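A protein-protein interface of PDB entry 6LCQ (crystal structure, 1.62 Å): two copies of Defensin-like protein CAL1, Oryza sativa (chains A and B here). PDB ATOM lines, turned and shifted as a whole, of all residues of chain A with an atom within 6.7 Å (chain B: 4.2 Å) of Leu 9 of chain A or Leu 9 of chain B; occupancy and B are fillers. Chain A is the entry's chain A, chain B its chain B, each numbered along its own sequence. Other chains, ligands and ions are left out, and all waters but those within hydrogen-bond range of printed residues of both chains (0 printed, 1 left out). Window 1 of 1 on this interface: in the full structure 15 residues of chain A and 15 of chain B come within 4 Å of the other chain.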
ATOM      1  N   HIS A   7     -30.664  19.613 -26.858  1.00  0.00           N
ATOM      2  CA  HIS A   7     -30.950  18.763 -25.704  1.00  0.00           C
ATOM      3  C   HIS A   7     -29.833  18.821 -24.691  1.00  0.00           C
ATOM      4  O   HIS A   7     -28.675  19.073 -25.034  1.00  0.00           O
ATOM      5  CB  HIS A   7     -31.197  17.316 -26.123  1.00  0.00           C
ATOM      6  CG  HIS A   7     -32.461  17.138 -26.900  1.00  0.00           C
ATOM      7  ND1 HIS A   7     -32.478  17.050 -28.274  1.00  0.00           N
ATOM      8  CD2 HIS A   7     -33.753  17.079 -26.503  1.00  0.00           C
ATOM      9  CE1 HIS A   7     -33.726  16.923 -28.688  1.00  0.00           C
ATOM     10  NE2 HIS A   7     -34.520  16.926 -27.634  1.00  0.00           N
ATOM     11  N   CYS A   8     -30.224  18.596 -23.442  1.00  0.00           N
ATOM     12  CA  CYS A   8     -29.353  18.683 -22.291  1.00  0.00           C
ATOM     13  C   CYS A   8     -29.430  17.348 -21.554  1.00  0.00           C
ATOM     14  O   CYS A   8     -30.501  16.721 -21.508  1.00  0.00           O
ATOM     15  CB  CYS A   8     -29.853  19.815 -21.402  1.00  0.00           C
ATOM     16  SG  CYS A   8     -29.143  21.444 -21.770  1.00  0.00           S
ATOM     17  N   LEU A   9     -28.315  16.949 -20.947  1.00  0.00           N
ATOM     18  CA  LEU A   9     -28.195  15.661 -20.261  1.00  0.00           C
ATOM     19  C   LEU A   9     -27.806  15.837 -18.810  1.00  0.00           C
ATOM     20  O   LEU A   9     -26.975  16.675 -18.483  1.00  0.00           O
ATOM     21  CB  LEU A   9     -27.122  14.799 -20.918  1.00  0.00           C
ATOM     22  CG  LEU A   9     -27.388  14.278 -22.324  1.00  0.00           C
ATOM     23  CD1 LEU A   9     -26.184  13.514 -22.840  1.00  0.00           C
ATOM     24  CD2 LEU A   9     -28.615  13.384 -22.308  1.00  0.00           C
ATOM     25  N   SER A  10     -28.374  14.996 -17.951  1.00  0.00           N
ATOM     26  CA  SER A  10     -28.071  15.031 -16.525  1.00  0.00           C
ATOM     27  C   SER A  10     -28.042  13.592 -16.028  1.00  0.00           C
ATOM     28  O   SER A  10     -29.020  12.858 -16.166  1.00  0.00           O
ATOM     29  CB  SER A  10     -29.122  15.854 -15.779  1.00  0.00           C
ATOM     30  OG  SER A  10     -28.875  15.856 -14.381  1.00  0.00           O
ATOM     31  N   GLN A  11     -26.929  13.182 -15.441  1.00  0.00           N
ATOM     32  CA  GLN A  11     -26.812  11.828 -14.942  1.00  0.00           C
ATOM     33  C   GLN A  11     -27.933  11.525 -13.952  1.00  0.00           C
ATOM     34  O   GLN A  11     -28.253  12.338 -13.064  1.00  0.00           O
ATOM     35  CB  GLN A  11     -25.447  11.606 -14.303  1.00  0.00           C
ATOM     36  CG  GLN A  11     -25.173  10.149 -14.018  1.00  0.00           C
ATOM     37  CD  GLN A  11     -23.714   9.864 -13.698  1.00  0.00           C
ATOM     38  OE1 GLN A  11     -22.803  10.544 -14.184  1.00  0.00           O
ATOM     39  NE2 GLN A  11     -23.488   8.834 -12.909  1.00  0.00           N
ATOM     40  N   PHE A  34     -37.911  13.887 -16.199  1.00  0.00           N
ATOM     41  CA  PHE A  34     -37.340  14.107 -17.525  1.00  0.00           C
ATOM     42  C   PHE A  34     -38.139  13.310 -18.538  1.00  0.00           C
ATOM     43  O   PHE A  34     -38.613  12.232 -18.226  1.00  0.00           O
ATOM     44  CB  PHE A  34     -35.879  13.639 -17.622  1.00  0.00           C
ATOM     45  CG  PHE A  34     -34.895  14.516 -16.912  1.00  0.00           C
ATOM     46  CD1 PHE A  34     -34.041  15.355 -17.619  1.00  0.00           C
ATOM     47  CD2 PHE A  34     -34.788  14.464 -15.538  1.00  0.00           C
ATOM     48  CE1 PHE A  34     -33.108  16.148 -16.961  1.00  0.00           C
ATOM     49  CE2 PHE A  34     -33.865  15.248 -14.878  1.00  0.00           C
ATOM     50  CZ  PHE A  34     -33.022  16.081 -15.590  1.00  0.00           C
ATOM     51  N   GLY A  37     -34.225   9.627 -21.747  1.00  0.00           N
ATOM     52  CA  GLY A  37     -32.933   9.265 -21.157  1.00  0.00           C
ATOM     53  C   GLY A  37     -32.212   8.273 -22.034  1.00  0.00           C
ATOM     54  O   GLY A  37     -32.814   7.623 -22.902  1.00  0.00           O
ATOM     55  N   GLU A  38     -30.912   8.130 -21.813  1.00  0.00           N
ATOM     56  CA  GLU A  38     -30.110   7.226 -22.628  1.00  0.00           C
ATOM     57  C   GLU A  38     -28.841   6.816 -21.892  1.00  0.00           C
ATOM     58  O   GLU A  38     -28.326   7.559 -21.052  1.00  0.00           O
ATOM     59  CB  GLU A  38     -29.768   7.897 -23.959  1.00  0.00           C
ATOM     60  CG  GLU A  38     -28.868   9.118 -23.844  1.00  0.00           C
ATOM     61  CD  GLU A  38     -28.879  10.019 -25.076  1.00  0.00           C
ATOM     62  OE1 GLU A  38     -29.811   9.953 -25.896  1.00  0.00           O
ATOM     63  OE2 GLU A  38     -27.952  10.825 -25.206  1.00  0.00           O
ATOM     64  N   LYS A  40     -24.884   6.088 -21.601  1.00  0.00           N
ATOM     65  CA  LYS A  40     -23.627   6.591 -22.163  1.00  0.00           C
ATOM     66  C   LYS A  40     -22.463   5.978 -21.419  1.00  0.00           C
ATOM     67  O   LYS A  40     -22.537   5.753 -20.212  1.00  0.00           O
ATOM     68  CB  LYS A  40     -23.551   8.110 -22.073  1.00  0.00           C
ATOM     69  CG  LYS A  40     -24.629   8.829 -22.861  1.00  0.00           C
ATOM     70  CD  LYS A  40     -24.074  10.037 -23.596  1.00  0.00           C
ATOM     71  CE  LYS A  40     -24.933  10.408 -24.785  1.00  0.00           C
ATOM     72  NZ  LYS A  40     -24.106  10.609 -26.001  1.00  0.00           N
ATOM     73  N   PHE A  49     -28.201   8.664 -18.425  1.00  0.00           N
ATOM     74  CA  PHE A  49     -28.303  10.128 -18.492  1.00  0.00           C
ATOM     75  C   PHE A  49     -29.694  10.527 -18.899  1.00  0.00           C
ATOM     76  O   PHE A  49     -30.171  10.144 -19.966  1.00  0.00           O
ATOM     77  CB  PHE A  49     -27.297  10.712 -19.481  1.00  0.00           C
ATOM     78  CG  PHE A  49     -25.895  10.633 -18.973  1.00  0.00           C
ATOM     79  CD1 PHE A  49     -25.296  11.723 -18.377  1.00  0.00           C
ATOM     80  CD2 PHE A  49     -25.217   9.422 -19.001  1.00  0.00           C
ATOM     81  CE1 PHE A  49     -24.002  11.629 -17.877  1.00  0.00           C
ATOM     82  CE2 PHE A  49     -23.934   9.323 -18.481  1.00  0.00           C
ATOM     83  CZ  PHE A  49     -23.336  10.426 -17.923  1.00  0.00           C
ATOM     84  N   CYS A  50     -30.343  11.303 -18.041  1.00  0.00           N
ATOM     85  CA  CYS A  50     -31.664  11.826 -18.356  1.00  0.00           C
ATOM     86  C   CYS A  50     -31.527  12.972 -19.336  1.00  0.00           C
ATOM     87  O   CYS A  50     -30.513  13.662 -19.369  1.00  0.00           O
ATOM     88  CB  CYS A  50     -32.373  12.263 -17.080  1.00  0.00           C
ATOM     89  SG  CYS A  50     -32.566  10.926 -15.879  1.00  0.00           S
ATOM     90  N   LYS A  51     -32.559  13.151 -20.151  1.00  0.00           N
ATOM     91  CA  LYS A  51     -32.458  13.993 -21.339  1.00  0.00           C
ATOM     92  C   LYS A  51     -33.715  14.838 -21.505  1.00  0.00           C
ATOM     93  O   LYS A  51     -34.830  14.335 -21.468  1.00  0.00           O
ATOM     94  CB  LYS A  51     -32.229  13.109 -22.564  1.00  0.00           C
ATOM     95  CG  LYS A  51     -32.002  13.867 -23.866  1.00  0.00           C
ATOM     96  CD  LYS A  51     -31.649  12.917 -25.005  1.00  0.00           C
ATOM     97  CE  LYS A  51     -31.233  13.660 -26.253  1.00  0.00           C
ATOM     98  NZ  LYS A  51     -30.970  12.711 -27.383  1.00  0.00           N
ATOM     99  N   LYS A  52     -33.507  16.132 -21.669  1.00  0.00           N
ATOM    100  CA  LYS A  52     -34.603  17.076 -21.897  1.00  0.00           C
ATOM    101  C   LYS A  52     -34.161  18.138 -22.890  1.00  0.00           C
ATOM    102  O   LYS A  52     -32.994  18.214 -23.258  1.00  0.00           O
ATOM    103  CB  LYS A  52     -35.034  17.717 -20.572  1.00  0.00           C
ATOM    104  CG  LYS A  52     -34.026  18.647 -19.916  1.00  0.00           C
ATOM    105  CD  LYS A  52     -34.555  19.248 -18.612  1.00  0.00           C
ATOM    106  CE  LYS A  52     -35.590  20.338 -18.849  1.00  0.00           C
ATOM    107  NZ  LYS A  52     -35.011  21.606 -19.366  1.00  0.00           N
ATOM    108  N   CYS A  54     -32.995  21.744 -23.602  1.00  0.00           N
ATOM    109  CA  CYS A  54     -32.320  22.676 -22.699  1.00  0.00           C
ATOM    110  C   CYS A  54     -33.233  23.805 -22.233  1.00  0.00           C
ATOM    111  O   CYS A  54     -34.056  24.325 -22.996  1.00  0.00           O
ATOM    112  CB  CYS A  54     -31.067  23.252 -23.336  1.00  0.00           C
ATOM    113  SG  CYS A  54     -29.795  22.019 -23.630  1.00  0.00           S
ATOM    114  OXT CYS A  54     -33.180  24.185 -21.059  1.00  0.00           O
ATOM    115  N   HIS B   7     -27.872  19.937 -12.381  1.00  0.00           N
ATOM    116  CA  HIS B   7     -27.271  20.519 -13.596  1.00  0.00           C
ATOM    117  C   HIS B   7     -27.373  19.652 -14.836  1.00  0.00           C
ATOM    118  O   HIS B   7     -27.376  18.429 -14.773  1.00  0.00           O
ATOM    119  CB  HIS B   7     -25.805  20.857 -13.371  1.00  0.00           C
ATOM    120  CG  HIS B   7     -25.610  21.901 -12.331  1.00  0.00           C
ATOM    121  ND1 HIS B   7     -25.802  23.239 -12.588  1.00  0.00           N
ATOM    122  CD2 HIS B   7     -25.292  21.805 -11.019  1.00  0.00           C
ATOM    123  CE1 HIS B   7     -25.585  23.930 -11.484  1.00  0.00           C
ATOM    124  NE2 HIS B   7     -25.279  23.083 -10.516  1.00  0.00           N
ATOM    125  N   CYS B   8     -27.449  20.347 -15.963  1.00  0.00           N
ATOM    126  CA  CYS B   8     -27.646  19.770 -17.275  1.00  0.00           C
ATOM    127  C   CYS B   8     -26.476  20.192 -18.191  1.00  0.00           C
ATOM    128  O   CYS B   8     -26.024  21.338 -18.137  1.00  0.00           O
ATOM    129  CB  CYS B   8     -28.995  20.278 -17.803  1.00  0.00           C
ATOM    130  SG  CYS B   8     -30.395  19.201 -17.348  1.00  0.00           S
ATOM    131  N   LEU B   9     -25.994  19.271 -19.028  1.00  0.00           N
ATOM    132  CA  LEU B   9     -24.892  19.547 -19.955  1.00  0.00           C
ATOM    133  C   LEU B   9     -25.302  19.383 -21.407  1.00  0.00           C
ATOM    134  O   LEU B   9     -26.068  18.487 -21.736  1.00  0.00           O
ATOM    135  CB  LEU B   9     -23.745  18.562 -19.713  1.00  0.00           C
ATOM    136  CG  LEU B   9     -22.984  18.602 -18.390  1.00  0.00           C
ATOM    137  CD1 LEU B   9     -21.971  17.477 -18.330  1.00  0.00           C
ATOM    138  CD2 LEU B   9     -22.298  19.930 -18.185  1.00  0.00           C
ATOM    139  N   SER B  10     -24.717  20.213 -22.269  1.00  0.00           N
ATOM    140  CA  SER B  10     -24.952  20.144 -23.707  1.00  0.00           C
ATOM    141  C   SER B  10     -23.662  20.490 -24.431  1.00  0.00           C
ATOM    142  O   SER B  10     -23.079  21.542 -24.204  1.00  0.00           O
ATOM    143  CB  SER B  10     -26.071  21.098 -24.110  1.00  0.00           C
ATOM    144  OG  SER B  10     -26.319  21.021 -25.507  1.00  0.00           O
ATOM    145  N   GLU B  38     -17.579  23.155 -19.138  1.00  0.00           N
ATOM    146  CA  GLU B  38     -16.388  22.413 -18.727  1.00  0.00           C
ATOM    147  C   GLU B  38     -15.949  21.463 -19.826  1.00  0.00           C
ATOM    148  O   GLU B  38     -16.770  21.005 -20.636  1.00  0.00           O
ATOM    149  CB  GLU B  38     -16.664  21.640 -17.443  1.00  0.00           C
ATOM    150  CG  GLU B  38     -17.755  20.588 -17.577  1.00  0.00           C
ATOM    151  CD  GLU B  38     -18.400  20.184 -16.262  1.00  0.00           C
ATOM    152  OE1 GLU B  38     -18.148  20.830 -15.217  1.00  0.00           O
ATOM    153  OE2 GLU B  38     -19.170  19.202 -16.284  1.00  0.00           O
ATOM    154  N   LYS B  40     -14.760  17.819 -21.095  1.00  0.00           N
ATOM    155  CA  LYS B  40     -14.899  16.404 -20.710  1.00  0.00           C
ATOM    156  C   LYS B  40     -14.255  15.528 -21.759  1.00  0.00           C
ATOM    157  O   LYS B  40     -14.285  15.851 -22.937  1.00  0.00           O
ATOM    158  CB  LYS B  40     -16.363  16.021 -20.576  1.00  0.00           C
ATOM    159  CG  LYS B  40     -17.108  16.856 -19.557  1.00  0.00           C
ATOM    160  CD  LYS B  40     -18.477  16.297 -19.226  1.00  0.00           C
ATOM    161  CE  LYS B  40     -18.418  15.312 -18.079  1.00  0.00           C
ATOM    162  NZ  LYS B  40     -18.376  15.988 -16.752  1.00  0.00           N
ATOM    163  N   CYS B  50     -21.370  22.788 -22.371  1.00  0.00           N
ATOM    164  CA  CYS B  50     -22.008  23.899 -21.691  1.00  0.00           C
ATOM    165  C   CYS B  50     -22.897  23.368 -20.570  1.00  0.00           C
ATOM    166  O   CYS B  50     -23.444  22.269 -20.646  1.00  0.00           O
ATOM    167  CB  CYS B  50     -22.794  24.738 -22.699  1.00  0.00           C
ATOM    168  SG  CYS B  50     -21.771  25.378 -24.051  1.00  0.00           S
ATOM    169  N   LYS B  51     -23.031  24.163 -19.516  1.00  0.00           N
ATOM    170  CA  LYS B  51     -23.627  23.698 -18.272  1.00  0.00           C
ATOM    171  C   LYS B  51     -24.597  24.728 -17.739  1.00  0.00           C
ATOM    172  O   LYS B  51     -24.270  25.910 -17.664  1.00  0.00           O
ATOM    173  CB  LYS B  51     -22.521  23.437 -17.252  1.00  0.00           C
ATOM    174  CG  LYS B  51     -22.983  22.830 -15.939  1.00  0.00           C
ATOM    175  CD  LYS B  51     -21.791  22.380 -15.109  1.00  0.00           C
ATOM    176  CE  LYS B  51     -22.219  21.748 -13.806  1.00  0.00           C
ATOM    177  NZ  LYS B  51     -21.014  21.530 -12.958  1.00  0.00           N
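The backbone carbonyl oxygen of His 7 of chain A sits at hydrogen-bond distance from the side-chain hydroxyl of Ser 10 of chain B, 3.1 Å away. The backbone carbonyl oxygen (O) of His 7 of chain B is in hydrogen-bond range of the side-chain hydroxyl (OG) of Ser 10 of chain A (3.0 Å). O of Leu 9 of chain A sits at hydrogen-bond distance from N of Leu 9 of chain B.
O of Ser 10 of chain B lies within hydrogen-bond range of N of Cys 50 of chain B, at 2.8 Å. The side-chain amino group of Lys 52 of chain A is in salt-bridge range of the chain-end carboxylate of Cys 54 of chain A (3.6 Å). The backbone carbonyl oxygen (O) of Lys 52 of chain A sits at hydrogen-bond distance from the backbone NH (N) of Cys 8 of chain A, 2.8 Å away. O of Ser 10 of chain A is in hydrogen-bond range of N of Cys 50 of chain A, 2.8 Å away. SG of Cys 8 of chain A is disulfide-bonded to SG of Cys 54 of chain A (2.1 Å).
CB of Cys 8 of chain B touches CB of Cys 8 of chain A, 3.7 Å away. Leu 9 of chain B touches Cys 8 of chain A. Ser 10 of chain B touches Cys 8 of chain A (CB to SG, 3.9 Å). Cys 8 of chain B touches Leu 9 of chain A. Cys 8 of chain B touches Ser 10 of chain A. SG of Cys 54 of chain A touches CB of Ser 10 of chain B, 3.9 Å away.
Of chain B, only Cys 8 and Leu 9 come within 4 Å of Leu 9 of chain A. Of the printed residues of chain A, Leu 9 of chain B touches Cys 8 and Leu 9. Printed residues of chain B within 4 Å of Cys 54 of chain A: Ser 10. Of the printed residues of chain B, His 7 of chain A touches Ser 10 (3.1 Å). Of the printed residues of chain A, His 7 of chain B touches Ser 10. Of the printed residues of chain B, Cys 8 of chain A touches Cys 8, Leu 9 and Ser 10. Lys 51 of chain B touches none of the printed residues of chain A. Cys 50 of chain B touches none of the printed residues of chain A. The nearest residue of chain B that does not touch Leu 9 of chain A is His 7 of chain B (4.1 Å).
Hydrophobic or aromatic side chains of chain A that line the printed part of chain B: Leu 9. Of the 8 printed residues of chain B, 4 touch a printed residue of chain A. Hydrophobic or aromatic side chains of chain B within 4 Å of the printed part of chain A: Leu 9. Among the printed residues, 9 pairs touch across the chains.
Cys 8 of chain B touches its own counterpart, Cys 8 of chain A. Cys 8 of chain A touches Leu 9 of chain B, and with the chains exchanged Leu 9 of chain A touches Cys 8 of chain B. Cys 8 of chain A touches Ser 10 of chain B, and with the chains exchanged Ser 10 of chain A touches Cys 8 of chain B. Leu 9 of chain B touches its own counterpart, Leu 9 of chain A.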
